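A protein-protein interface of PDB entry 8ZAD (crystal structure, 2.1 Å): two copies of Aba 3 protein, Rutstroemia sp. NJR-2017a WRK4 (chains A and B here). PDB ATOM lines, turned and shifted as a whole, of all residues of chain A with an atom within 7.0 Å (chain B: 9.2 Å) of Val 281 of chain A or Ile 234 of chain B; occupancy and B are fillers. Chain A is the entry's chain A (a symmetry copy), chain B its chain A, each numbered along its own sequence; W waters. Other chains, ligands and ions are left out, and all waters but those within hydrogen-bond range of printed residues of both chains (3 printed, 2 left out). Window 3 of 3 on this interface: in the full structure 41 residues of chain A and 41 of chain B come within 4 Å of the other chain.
NH1 of Arg 241 of chain B sits at hydrogen-bond distance from O of Met 273 of chain A (2.8 Å).
OH of Tyr 237 of chain B is in hydrogen-bond range of O of Met 273 of chain A, at 3.0 Å.
O of Phe 280 of chain A sits at hydrogen-bond distance from N of Leu 285 of chain A (2.8 Å).
The backbone carbonyl oxygen (O) of Ala 209 of chain B is in hydrogen-bond range of the guanidinium group (NH2) of Arg 233 of chain B.
Among the printed residues, pairs that only touch across the chains: Phe 280 of chain A with Tyr 237 of chain B (3.6 Å), Val 281 of chain A with Ile 234 of chain B (3.6 Å), Val 281 of chain A with Ser 238 of chain B (3.8 Å), Val 281 of chain A with Arg 241 of chain B (3.4 Å), Asn 284 of chain A with Ile 234 of chain B (3.7 Å), Leu 285 of chain A with Ala 209 of chain B (3.8 Å), Leu 285 of chain A with Ile 234 of chain B (3.6 Å) and Leu 285 of chain A with Tyr 237 of chain B (3.6 Å).
Of the printed residues of chain B, Met 273 of chain A touches Tyr 237 (3.0 Å) and Arg 241 (2.8 Å).
Of the printed residues of chain B, Val 281 of chain A touches Ile 234, Ser 238 and Arg 241.
No residue of chain B comes within 4 Å of Glu 282 of chain A.
Of the printed residues of chain B, Asn 284 of chain A touches Ile 234.
Of the printed residues of chain B, Leu 285 of chain A touches Ala 209, Ile 234 and Tyr 237.
Thr 205 of chain B touches none of the printed residues of chain A.
Of the printed residues of chain A, Ala 209 of chain B touches Leu 285 (3.8 Å).
Of chain A, only Val 281 (3.6 Å), Asn 284 (3.7 Å) and Leu 285 (3.6 Å) come within 4 Å of Ile 234 of chain B.
Printed residues of chain A within 4 Å of Ser 238 of chain B: Val 281 (3.8 Å).
The nearest residue of chain A that does not touch Ile 234 of chain B is Glu 282 of chain A (5.7 Å).
The nearest printed residue of chain A that does not touch Tyr 237 of chain B is Val 281 of chain A (4.01 Å).
Of the 11 printed residues of chain A, 5 touch a printed residue of chain B.
Printed residues of chain B that touch a printed residue of chain A: Ala 209, Ile 234, Tyr 237, Ser 238 and Arg 241.
Hydrophobic or aromatic side chains of chain B within 4 Å of the printed part of chain A: Ala 209, Ile 234 and Tyr 237.
Among the printed residues, no Asp or Glu carboxylate lies within 4 Å of a Lys or Arg side-chain nitrogen of the other chain.
No position is printed for both chains.
Water W1 bridges the backbone carbonyl oxygen (O) of Asn 284 of chain A (2.4 Å) and the guanidinium group (NH1) of Arg 233 of chain B (3.2 Å).
Water W2 lies within hydrogen-bond range of the backbone carbonyl oxygen (O) of His 272 of chain A, the guanidinium group (NH1) of Arg 241 of chain B, the backbone NH (N) of Phe 280 of chain A and the backbone carbonyl oxygen (O) of Tyr 278 of chain A.
Water W3 lies within hydrogen-bond range of NH2 of Arg 233 of chain B, O of Leu 285 of chain A and O of Asn 284 of chain A.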
ATOM      1  N   HIS A 272     -20.567  34.519 -17.659  1.00  0.00           N
ATOM      2  CA  HIS A 272     -21.976  34.052 -17.821  1.00  0.00           C
ATOM      3  C   HIS A 272     -21.949  32.577 -18.249  1.00  0.00           C
ATOM      4  O   HIS A 272     -22.804  31.819 -17.815  1.00  0.00           O
ATOM      5  CB  HIS A 272     -22.759  34.954 -18.790  1.00  0.00           C
ATOM      6  CG  HIS A 272     -22.985  36.344 -18.278  1.00  0.00           C
ATOM      7  ND1 HIS A 272     -24.215  36.778 -17.822  1.00  0.00           N
ATOM      8  CD2 HIS A 272     -22.160  37.420 -18.188  1.00  0.00           C
ATOM      9  CE1 HIS A 272     -24.137  38.039 -17.439  1.00  0.00           C
ATOM     10  NE2 HIS A 272     -22.884  38.469 -17.680  1.00  0.00           N
ATOM     11  N   MET A 273     -20.944  32.152 -19.010  1.00  0.00           N
ATOM     12  CA  MET A 273     -20.841  30.732 -19.433  1.00  0.00           C
ATOM     13  C   MET A 273     -20.172  29.837 -18.369  1.00  0.00           C
ATOM     14  O   MET A 273     -20.434  28.625 -18.377  1.00  0.00           O
ATOM     15  CB  MET A 273     -20.055  30.633 -20.732  1.00  0.00           C
ATOM     16  CG  MET A 273     -20.688  31.445 -21.846  1.00  0.00           C
ATOM     17  SD  MET A 273     -19.923  31.221 -23.455  1.00  0.00           S
ATOM     18  CE  MET A 273     -19.696  29.458 -23.469  1.00  0.00           C
ATOM     19  N   TYR A 278     -24.722  31.837 -12.837  1.00  0.00           N
ATOM     20  CA  TYR A 278     -25.464  32.325 -14.025  1.00  0.00           C
ATOM     21  C   TYR A 278     -26.274  31.137 -14.567  1.00  0.00           C
ATOM     22  O   TYR A 278     -26.193  29.985 -14.003  1.00  0.00           O
ATOM     23  CB  TYR A 278     -24.530  32.987 -15.038  1.00  0.00           C
ATOM     24  CG  TYR A 278     -23.840  34.220 -14.510  1.00  0.00           C
ATOM     25  CD1 TYR A 278     -24.501  35.440 -14.419  1.00  0.00           C
ATOM     26  CD2 TYR A 278     -22.530  34.162 -14.063  1.00  0.00           C
ATOM     27  CE1 TYR A 278     -23.865  36.571 -13.922  1.00  0.00           C
ATOM     28  CE2 TYR A 278     -21.882  35.280 -13.555  1.00  0.00           C
ATOM     29  CZ  TYR A 278     -22.545  36.495 -13.499  1.00  0.00           C
ATOM     30  OH  TYR A 278     -21.905  37.591 -13.005  1.00  0.00           O
ATOM     31  N   ARG A 279     -27.063  31.414 -15.596  1.00  0.00           N
ATOM     32  CA  ARG A 279     -28.191  30.562 -16.025  1.00  0.00           C
ATOM     33  C   ARG A 279     -27.952  30.033 -17.441  1.00  0.00           C
ATOM     34  O   ARG A 279     -28.889  29.535 -18.022  1.00  0.00           O
ATOM     35  CB  ARG A 279     -29.475  31.384 -15.889  1.00  0.00           C
ATOM     36  CG  ARG A 279     -29.778  31.774 -14.446  1.00  0.00           C
ATOM     37  CD  ARG A 279     -31.249  31.977 -14.075  1.00  0.00           C
ATOM     38  NE  ARG A 279     -32.198  31.853 -15.183  1.00  0.00           N
ATOM     39  CZ  ARG A 279     -33.022  30.822 -15.383  1.00  0.00           C
ATOM     40  NH1 ARG A 279     -33.044  29.796 -14.542  1.00  0.00           N
ATOM     41  NH2 ARG A 279     -33.838  30.836 -16.422  1.00  0.00           N
ATOM     42  N   PHE A 280     -26.713  30.055 -17.931  1.00  0.00           N
ATOM     43  CA  PHE A 280     -26.350  29.544 -19.277  1.00  0.00           C
ATOM     44  C   PHE A 280     -27.013  28.174 -19.527  1.00  0.00           C
ATOM     45  O   PHE A 280     -27.617  27.987 -20.599  1.00  0.00           O
ATOM     46  CB  PHE A 280     -24.825  29.486 -19.412  1.00  0.00           C
ATOM     47  CG  PHE A 280     -24.350  29.206 -20.807  1.00  0.00           C
ATOM     48  CD1 PHE A 280     -24.786  29.980 -21.873  1.00  0.00           C
ATOM     49  CD2 PHE A 280     -23.476  28.160 -21.055  1.00  0.00           C
ATOM     50  CE1 PHE A 280     -24.357  29.715 -23.168  1.00  0.00           C
ATOM     51  CE2 PHE A 280     -23.061  27.886 -22.348  1.00  0.00           C
ATOM     52  CZ  PHE A 280     -23.479  28.673 -23.401  1.00  0.00           C
ATOM     53  N   VAL A 281     -26.860  27.231 -18.604  1.00  0.00           N
ATOM     54  CA  VAL A 281     -27.401  25.845 -18.718  1.00  0.00           C
ATOM     55  C   VAL A 281     -28.931  25.923 -18.719  1.00  0.00           C
ATOM     56  O   VAL A 281     -29.552  25.266 -19.592  1.00  0.00           O
ATOM     57  CB  VAL A 281     -26.871  24.919 -17.599  1.00  0.00           C
ATOM     58  CG1 VAL A 281     -27.637  23.599 -17.498  1.00  0.00           C
ATOM     59  CG2 VAL A 281     -25.390  24.621 -17.800  1.00  0.00           C
ATOM     60  N   GLU A 282     -29.501  26.687 -17.780  1.00  0.00           N
ATOM     61  CA  GLU A 282     -30.966  26.790 -17.567  1.00  0.00           C
ATOM     62  C   GLU A 282     -31.597  27.422 -18.801  1.00  0.00           C
ATOM     63  O   GLU A 282     -32.737  27.127 -19.079  1.00  0.00           O
ATOM     64  CB  GLU A 282     -31.293  27.582 -16.303  1.00  0.00           C
ATOM     65  CG  GLU A 282     -30.874  26.867 -15.033  1.00  0.00           C
ATOM     66  CD  GLU A 282     -29.402  26.952 -14.617  1.00  0.00           C
ATOM     67  OE1 GLU A 282     -29.112  26.381 -13.570  1.00  0.00           O
ATOM     68  OE2 GLU A 282     -28.553  27.598 -15.323  1.00  0.00           O
ATOM     69  N   GLU A 283     -30.854  28.205 -19.575  1.00  0.00           N
ATOM     70  CA  GLU A 283     -31.397  28.784 -20.825  1.00  0.00           C
ATOM     71  C   GLU A 283     -30.911  28.005 -22.043  1.00  0.00           C
ATOM     72  O   GLU A 283     -30.965  28.565 -23.152  1.00  0.00           O
ATOM     73  CB  GLU A 283     -31.033  30.255 -20.869  1.00  0.00           C
ATOM     74  CG  GLU A 283     -31.368  30.927 -19.562  1.00  0.00           C
ATOM     75  CD  GLU A 283     -31.546  32.422 -19.672  1.00  0.00           C
ATOM     76  OE1 GLU A 283     -31.050  33.008 -20.665  1.00  0.00           O
ATOM     77  OE2 GLU A 283     -32.205  32.983 -18.770  1.00  0.00           O
ATOM     78  N   ASN A 284     -30.467  26.764 -21.842  1.00  0.00           N
ATOM     79  CA  ASN A 284     -30.220  25.760 -22.921  1.00  0.00           C
ATOM     80  C   ASN A 284     -28.981  26.183 -23.708  1.00  0.00           C
ATOM     81  O   ASN A 284     -28.977  26.054 -24.933  1.00  0.00           O
ATOM     82  CB  ASN A 284     -31.463  25.549 -23.796  1.00  0.00           C
ATOM     83  CG  ASN A 284     -32.635  25.071 -22.966  1.00  0.00           C
ATOM     84  OD1 ASN A 284     -32.503  24.132 -22.199  1.00  0.00           O
ATOM     85  ND2 ASN A 284     -33.750  25.776 -23.022  1.00  0.00           N
ATOM     86  N   LEU A 285     -27.961  26.649 -22.992  1.00  0.00           N
ATOM     87  CA  LEU A 285     -26.664  27.089 -23.565  1.00  0.00           C
ATOM     88  C   LEU A 285     -26.974  28.223 -24.544  1.00  0.00           C
ATOM     89  O   LEU A 285     -26.493  28.192 -25.684  1.00  0.00           O
ATOM     90  CB  LEU A 285     -25.949  25.900 -24.223  1.00  0.00           C
ATOM     91  CG  LEU A 285     -25.877  24.620 -23.381  1.00  0.00           C
ATOM     92  CD1 LEU A 285     -25.037  23.557 -24.058  1.00  0.00           C
ATOM     93  CD2 LEU A 285     -25.332  24.874 -21.994  1.00  0.00           C
ATOM     94  N   THR A 286     -27.812  29.167 -24.133  1.00  0.00           N
ATOM     95  CA  THR A 286     -28.031  30.415 -24.906  1.00  0.00           C
ATOM     96  C   THR A 286     -27.678  31.624 -24.033  1.00  0.00           C
ATOM     97  O   THR A 286     -27.737  31.518 -22.785  1.00  0.00           O
ATOM     98  CB  THR A 286     -29.441  30.529 -25.523  1.00  0.00           C
ATOM     99  OG1 THR A 286     -30.396  30.727 -24.484  1.00  0.00           O
ATOM    100  CG2 THR A 286     -29.810  29.332 -26.375  1.00  0.00           C
ATOM    101  N   THR B 205     -16.343  18.312 -25.378  1.00  0.00           N
ATOM    102  CA  THR B 205     -17.801  18.207 -25.155  1.00  0.00           C
ATOM    103  C   THR B 205     -18.317  19.624 -24.886  1.00  0.00           C
ATOM    104  O   THR B 205     -19.336  20.057 -25.523  1.00  0.00           O
ATOM    105  CB  THR B 205     -18.128  17.207 -24.044  1.00  0.00           C
ATOM    106  OG1 THR B 205     -17.609  15.935 -24.446  1.00  0.00           O
ATOM    107  CG2 THR B 205     -19.616  17.136 -23.766  1.00  0.00           C
ATOM    108  N   LEU B 206     -17.612  20.368 -24.029  1.00  0.00           N
ATOM    109  CA  LEU B 206     -18.017  21.769 -23.691  1.00  0.00           C
ATOM    110  C   LEU B 206     -18.078  22.592 -24.982  1.00  0.00           C
ATOM    111  O   LEU B 206     -19.120  23.164 -25.279  1.00  0.00           O
ATOM    112  CB  LEU B 206     -17.028  22.369 -22.691  1.00  0.00           C
ATOM    113  CG  LEU B 206     -17.149  21.860 -21.257  1.00  0.00           C
ATOM    114  CD1 LEU B 206     -15.958  22.349 -20.445  1.00  0.00           C
ATOM    115  CD2 LEU B 206     -18.461  22.315 -20.603  1.00  0.00           C
ATOM    116  N   ASP B 208     -18.122  21.656 -28.246  1.00  0.00           N
ATOM    117  CA  ASP B 208     -19.046  21.098 -29.262  1.00  0.00           C
ATOM    118  C   ASP B 208     -20.516  21.300 -28.863  1.00  0.00           C
ATOM    119  O   ASP B 208     -21.373  21.515 -29.792  1.00  0.00           O
ATOM    120  CB  ASP B 208     -18.708  19.632 -29.540  1.00  0.00           C
ATOM    121  CG  ASP B 208     -17.480  19.499 -30.418  1.00  0.00           C
ATOM    122  OD1 ASP B 208     -17.002  20.557 -30.870  1.00  0.00           O
ATOM    123  OD2 ASP B 208     -17.065  18.336 -30.695  1.00  0.00           O
ATOM    124  N   ALA B 209     -20.829  21.287 -27.570  1.00  0.00           N
ATOM    125  CA  ALA B 209     -22.199  21.587 -27.097  1.00  0.00           C
ATOM    126  C   ALA B 209     -22.541  23.021 -27.502  1.00  0.00           C
ATOM    127  O   ALA B 209     -23.691  23.260 -27.978  1.00  0.00           O
ATOM    128  CB  ALA B 209     -22.371  21.352 -25.614  1.00  0.00           C
ATOM    129  N   VAL B 210     -21.582  23.934 -27.385  1.00  0.00           N
ATOM    130  CA  VAL B 210     -21.802  25.378 -27.684  1.00  0.00           C
ATOM    131  C   VAL B 210     -21.719  25.595 -29.194  1.00  0.00           C
ATOM    132  O   VAL B 210     -22.496  26.413 -29.689  1.00  0.00           O
ATOM    133  CB  VAL B 210     -20.836  26.279 -26.895  1.00  0.00           C
ATOM    134  CG1 VAL B 210     -20.937  27.740 -27.308  1.00  0.00           C
ATOM    135  CG2 VAL B 210     -21.087  26.153 -25.395  1.00  0.00           C
ATOM    136  N   PHE B 212     -22.558  23.708 -31.567  1.00  0.00           N
ATOM    137  CA  PHE B 212     -23.596  22.809 -32.141  1.00  0.00           C
ATOM    138  C   PHE B 212     -24.281  23.434 -33.365  1.00  0.00           C
ATOM    139  O   PHE B 212     -24.238  22.814 -34.435  1.00  0.00           O
ATOM    140  CB  PHE B 212     -24.635  22.421 -31.088  1.00  0.00           C
ATOM    141  CG  PHE B 212     -25.747  21.556 -31.621  1.00  0.00           C
ATOM    142  CD1 PHE B 212     -25.502  20.256 -32.026  1.00  0.00           C
ATOM    143  CD2 PHE B 212     -27.039  22.046 -31.742  1.00  0.00           C
ATOM    144  CE1 PHE B 212     -26.522  19.464 -32.543  1.00  0.00           C
ATOM    145  CE2 PHE B 212     -28.053  21.260 -32.279  1.00  0.00           C
ATOM    146  CZ  PHE B 212     -27.795  19.964 -32.664  1.00  0.00           C
ATOM    147  N   TYR B 213     -24.908  24.591 -33.203  1.00  0.00           N
ATOM    148  CA  TYR B 213     -25.727  25.236 -34.261  1.00  0.00           C
ATOM    149  C   TYR B 213     -24.823  25.688 -35.413  1.00  0.00           C
ATOM    150  O   TYR B 213     -25.118  25.338 -36.568  1.00  0.00           O
ATOM    151  CB  TYR B 213     -26.560  26.360 -33.651  1.00  0.00           C
ATOM    152  CG  TYR B 213     -27.750  25.840 -32.886  1.00  0.00           C
ATOM    153  CD1 TYR B 213     -28.672  25.013 -33.519  1.00  0.00           C
ATOM    154  CD2 TYR B 213     -27.955  26.156 -31.548  1.00  0.00           C
ATOM    155  CE1 TYR B 213     -29.764  24.497 -32.849  1.00  0.00           C
ATOM    156  CE2 TYR B 213     -29.050  25.647 -30.861  1.00  0.00           C
ATOM    157  CZ  TYR B 213     -29.958  24.818 -31.515  1.00  0.00           C
ATOM    158  OH  TYR B 213     -31.045  24.292 -30.865  1.00  0.00           O
ATOM    159  N   PHE B 225     -22.149  16.318 -31.078  1.00  0.00           N
ATOM    160  CA  PHE B 225     -23.603  16.050 -31.031  1.00  0.00           C
ATOM    161  C   PHE B 225     -24.174  15.875 -32.442  1.00  0.00           C
ATOM    162  O   PHE B 225     -25.402  15.995 -32.597  1.00  0.00           O
ATOM    163  CB  PHE B 225     -24.265  17.127 -30.179  1.00  0.00           C
ATOM    164  CG  PHE B 225     -23.808  16.992 -28.761  1.00  0.00           C
ATOM    165  CD1 PHE B 225     -24.349  16.020 -27.943  1.00  0.00           C
ATOM    166  CD2 PHE B 225     -22.760  17.757 -28.290  1.00  0.00           C
ATOM    167  CE1 PHE B 225     -23.892  15.851 -26.650  1.00  0.00           C
ATOM    168  CE2 PHE B 225     -22.328  17.602 -26.989  1.00  0.00           C
ATOM    169  CZ  PHE B 225     -22.870  16.632 -26.186  1.00  0.00           C
ATOM    170  N   PRO B 229     -26.376  11.928 -28.556  1.00  0.00           N
ATOM    171  CA  PRO B 229     -27.765  12.395 -28.590  1.00  0.00           C
ATOM    172  C   PRO B 229     -27.924  13.910 -28.406  1.00  0.00           C
ATOM    173  O   PRO B 229     -27.341  14.474 -27.453  1.00  0.00           O
ATOM    174  CB  PRO B 229     -28.418  11.724 -27.373  1.00  0.00           C
ATOM    175  CG  PRO B 229     -27.539  10.554 -27.085  1.00  0.00           C
ATOM    176  CD  PRO B 229     -26.135  10.967 -27.477  1.00  0.00           C
ATOM    177  N   GLU B 230     -28.721  14.532 -29.274  1.00  0.00           N
ATOM    178  CA  GLU B 230     -29.035  15.980 -29.196  1.00  0.00           C
ATOM    179  C   GLU B 230     -29.744  16.263 -27.881  1.00  0.00           C
ATOM    180  O   GLU B 230     -29.547  17.342 -27.351  1.00  0.00           O
ATOM    181  CB  GLU B 230     -29.916  16.451 -30.348  1.00  0.00           C
ATOM    182  CG  GLU B 230     -29.143  16.535 -31.637  1.00  0.00           C
ATOM    183  CD  GLU B 230     -29.945  16.962 -32.851  1.00  0.00           C
ATOM    184  OE1 GLU B 230     -29.506  16.639 -33.954  1.00  0.00           O
ATOM    185  OE2 GLU B 230     -30.974  17.648 -32.685  1.00  0.00           O
ATOM    186  N   ASP B 231     -30.549  15.321 -27.398  1.00  0.00           N
ATOM    187  CA  ASP B 231     -31.380  15.511 -26.192  1.00  0.00           C
ATOM    188  C   ASP B 231     -30.527  15.407 -24.919  1.00  0.00           C
ATOM    189  O   ASP B 231     -31.091  15.676 -23.854  1.00  0.00           O
ATOM    190  CB  ASP B 231     -32.551  14.539 -26.182  1.00  0.00           C
ATOM    191  CG  ASP B 231     -32.166  13.152 -25.730  1.00  0.00           C
ATOM    192  OD1 ASP B 231     -31.035  12.769 -25.938  1.00  0.00           O
ATOM    193  OD2 ASP B 231     -33.018  12.476 -25.160  1.00  0.00           O
ATOM    194  N   LEU B 232     -29.217  15.138 -25.018  1.00  0.00           N
ATOM    195  CA  LEU B 232     -28.261  15.151 -23.868  1.00  0.00           C
ATOM    196  C   LEU B 232     -27.210  16.279 -23.981  1.00  0.00           C
ATOM    197  O   LEU B 232     -26.358  16.379 -23.061  1.00  0.00           O
ATOM    198  CB  LEU B 232     -27.579  13.777 -23.789  1.00  0.00           C
ATOM    199  CG  LEU B 232     -28.471  12.624 -23.314  1.00  0.00           C
ATOM    200  CD1 LEU B 232     -27.685  11.323 -23.259  1.00  0.00           C
ATOM    201  CD2 LEU B 232     -29.112  12.925 -21.952  1.00  0.00           C
ATOM    202  N   ARG B 233     -27.251  17.103 -25.031  1.00  0.00           N
ATOM    203  CA  ARG B 233     -26.273  18.198 -25.256  1.00  0.00           C
ATOM    204  C   ARG B 233     -26.191  19.152 -24.044  1.00  0.00           C
ATOM    205  O   ARG B 233     -25.060  19.415 -23.575  1.00  0.00           O
ATOM    206  CB  ARG B 233     -26.639  19.000 -26.500  1.00  0.00           C
ATOM    207  CG  ARG B 233     -25.598  20.053 -26.846  1.00  0.00           C
ATOM    208  CD  ARG B 233     -25.880  20.701 -28.181  1.00  0.00           C
ATOM    209  NE  ARG B 233     -27.212  21.261 -28.206  1.00  0.00           N
ATOM    210  CZ  ARG B 233     -27.517  22.544 -28.011  1.00  0.00           C
ATOM    211  NH1 ARG B 233     -28.784  22.919 -28.086  1.00  0.00           N
ATOM    212  NH2 ARG B 233     -26.581  23.455 -27.764  1.00  0.00           N
ATOM    213  N   ILE B 234     -27.320  19.668 -23.567  1.00  0.00           N
ATOM    214  CA  ILE B 234     -27.392  20.650 -22.441  1.00  0.00           C
ATOM    215  C   ILE B 234     -26.809  20.002 -21.184  1.00  0.00           C
ATOM    216  O   ILE B 234     -25.949  20.610 -20.510  1.00  0.00           O
ATOM    217  CB  ILE B 234     -28.846  21.099 -22.194  1.00  0.00           C
ATOM    218  CG1 ILE B 234     -29.536  21.658 -23.441  1.00  0.00           C
ATOM    219  CG2 ILE B 234     -28.914  22.079 -21.038  1.00  0.00           C
ATOM    220  CD1 ILE B 234     -28.658  22.467 -24.314  1.00  0.00           C
ATOM    221  N   LYS B 235     -27.264  18.791 -20.876  1.00  0.00           N
ATOM    222  CA  LYS B 235     -26.831  18.032 -19.678  1.00  0.00           C
ATOM    223  C   LYS B 235     -25.325  17.718 -19.788  1.00  0.00           C
ATOM    224  O   LYS B 235     -24.619  17.764 -18.778  1.00  0.00           O
ATOM    225  CB  LYS B 235     -27.704  16.781 -19.532  1.00  0.00           C
ATOM    226  CG  LYS B 235     -27.396  15.960 -18.288  1.00  0.00           C
ATOM    227  CD  LYS B 235     -28.353  14.799 -18.021  1.00  0.00           C
ATOM    228  CE  LYS B 235     -27.823  13.918 -16.903  1.00  0.00           C
ATOM    229  NZ  LYS B 235     -28.873  13.556 -15.923  1.00  0.00           N
ATOM    230  N   ALA B 236     -24.833  17.404 -20.981  1.00  0.00           N
ATOM    231  CA  ALA B 236     -23.404  17.066 -21.194  1.00  0.00           C
ATOM    232  C   ALA B 236     -22.556  18.295 -20.845  1.00  0.00           C
ATOM    233  O   ALA B 236     -21.575  18.158 -20.100  1.00  0.00           O
ATOM    234  CB  ALA B 236     -23.172  16.603 -22.620  1.00  0.00           C
ATOM    235  N   TYR B 237     -22.954  19.476 -21.307  1.00  0.00           N
ATOM    236  CA  TYR B 237     -22.220  20.713 -20.977  1.00  0.00           C
ATOM    237  C   TYR B 237     -22.197  20.839 -19.458  1.00  0.00           C
ATOM    238  O   TYR B 237     -21.139  21.076 -18.854  1.00  0.00           O
ATOM    239  CB  TYR B 237     -22.851  21.930 -21.650  1.00  0.00           C
ATOM    240  CG  TYR B 237     -22.085  23.211 -21.416  1.00  0.00           C
ATOM    241  CD1 TYR B 237     -22.301  23.971 -20.270  1.00  0.00           C
ATOM    242  CD2 TYR B 237     -21.155  23.674 -22.341  1.00  0.00           C
ATOM    243  CE1 TYR B 237     -21.574  25.127 -20.014  1.00  0.00           C
ATOM    244  CE2 TYR B 237     -20.446  24.846 -22.114  1.00  0.00           C
ATOM    245  CZ  TYR B 237     -20.653  25.569 -20.947  1.00  0.00           C
ATOM    246  OH  TYR B 237     -19.968  26.729 -20.719  1.00  0.00           O
ATOM    247  N   SER B 238     -23.378  20.704 -18.855  1.00  0.00           N
ATOM    248  CA  SER B 238     -23.580  20.951 -17.413  1.00  0.00           C
ATOM    249  C   SER B 238     -22.683  19.995 -16.620  1.00  0.00           C
ATOM    250  O   SER B 238     -21.951  20.467 -15.733  1.00  0.00           O
ATOM    251  CB  SER B 238     -25.018  20.841 -17.037  1.00  0.00           C
ATOM    252  OG  SER B 238     -25.140  20.842 -15.631  1.00  0.00           O
ATOM    253  N   GLU B 239     -22.658  18.717 -16.994  1.00  0.00           N
ATOM    254  CA  GLU B 239     -21.855  17.699 -16.265  1.00  0.00           C
ATOM    255  C   GLU B 239     -20.352  17.906 -16.496  1.00  0.00           C
ATOM    256  O   GLU B 239     -19.575  17.784 -15.520  1.00  0.00           O
ATOM    257  CB  GLU B 239     -22.297  16.295 -16.664  1.00  0.00           C
ATOM    258  CG  GLU B 239     -23.637  15.914 -16.046  1.00  0.00           C
ATOM    259  CD  GLU B 239     -23.980  14.440 -16.192  1.00  0.00           C
ATOM    260  OE1 GLU B 239     -24.910  14.013 -15.525  1.00  0.00           O
ATOM    261  OE2 GLU B 239     -23.326  13.729 -17.009  1.00  0.00           O
ATOM    262  N   CYS B 240     -19.927  18.190 -17.726  1.00  0.00           N
ATOM    263  CA  CYS B 240     -18.501  18.447 -18.029  1.00  0.00           C
ATOM    264  C   CYS B 240     -18.046  19.674 -17.228  1.00  0.00           C
ATOM    265  O   CYS B 240     -16.957  19.638 -16.670  1.00  0.00           O
ATOM    266  CB  CYS B 240     -18.272  18.620 -19.524  1.00  0.00           C
ATOM    267  SG  CYS B 240     -18.406  17.053 -20.434  1.00  0.00           S
ATOM    268  N   ARG B 241     -18.880  20.699 -17.145  1.00  0.00           N
ATOM    269  CA  ARG B 241     -18.523  21.964 -16.459  1.00  0.00           C
ATOM    270  C   ARG B 241     -18.390  21.703 -14.956  1.00  0.00           C
ATOM    271  O   ARG B 241     -17.477  22.232 -14.316  1.00  0.00           O
ATOM    272  CB  ARG B 241     -19.571  23.031 -16.739  1.00  0.00           C
ATOM    273  CG  ARG B 241     -19.227  24.341 -16.061  1.00  0.00           C
ATOM    274  CD  ARG B 241     -20.136  25.423 -16.541  1.00  0.00           C
ATOM    275  NE  ARG B 241     -21.426  25.297 -15.868  1.00  0.00           N
ATOM    276  CZ  ARG B 241     -22.410  26.172 -15.994  1.00  0.00           C
ATOM    277  NH1 ARG B 241     -22.251  27.237 -16.765  1.00  0.00           N
ATOM    278  NH2 ARG B 241     -23.540  25.992 -15.329  1.00  0.00           N
ATOM    279  N   GLU B 242     -19.304  20.920 -14.406  1.00  0.00           N
ATOM    280  CA  GLU B 242     -19.278  20.577 -12.977  1.00  0.00           C
ATOM    281  C   GLU B 242     -18.044  19.724 -12.661  1.00  0.00           C
ATOM    282  O   GLU B 242     -17.349  19.985 -11.634  1.00  0.00           O
ATOM    283  CB  GLU B 242     -20.561  19.850 -12.613  1.00  0.00           C
ATOM    284  CG  GLU B 242     -20.626  19.628 -11.137  1.00  0.00           C
ATOM    285  CD  GLU B 242     -21.954  19.093 -10.641  1.00  0.00           C
ATOM    286  OE1 GLU B 242     -23.014  19.406 -11.266  1.00  0.00           O
ATOM    287  OE2 GLU B 242     -21.904  18.380  -9.644  1.00  0.00           O
ATOM    288  N   LEU B 383     -21.905   8.279 -23.145  1.00  0.00           N
ATOM    289  CA  LEU B 383     -22.099   9.653 -22.627  1.00  0.00           C
ATOM    290  C   LEU B 383     -22.685   9.620 -21.206  1.00  0.00           C
ATOM    291  O   LEU B 383     -22.207  10.373 -20.361  1.00  0.00           O
ATOM    292  CB  LEU B 383     -23.027  10.421 -23.555  1.00  0.00           C
ATOM    293  CG  LEU B 383     -23.134  11.906 -23.231  1.00  0.00           C
ATOM    294  CD1 LEU B 383     -21.745  12.544 -23.231  1.00  0.00           C
ATOM    295  CD2 LEU B 383     -24.064  12.594 -24.229  1.00  0.00           C
HETATM  296  O   HOH W   1     -29.803  25.776 -27.199  1.00  0.00           O
HETATM  297  O   HOH W   2     -23.769  29.777 -16.340  1.00  0.00           O
HETATM  298  O   HOH W   3     -27.462  26.284 -27.912  1.00  0.00           O
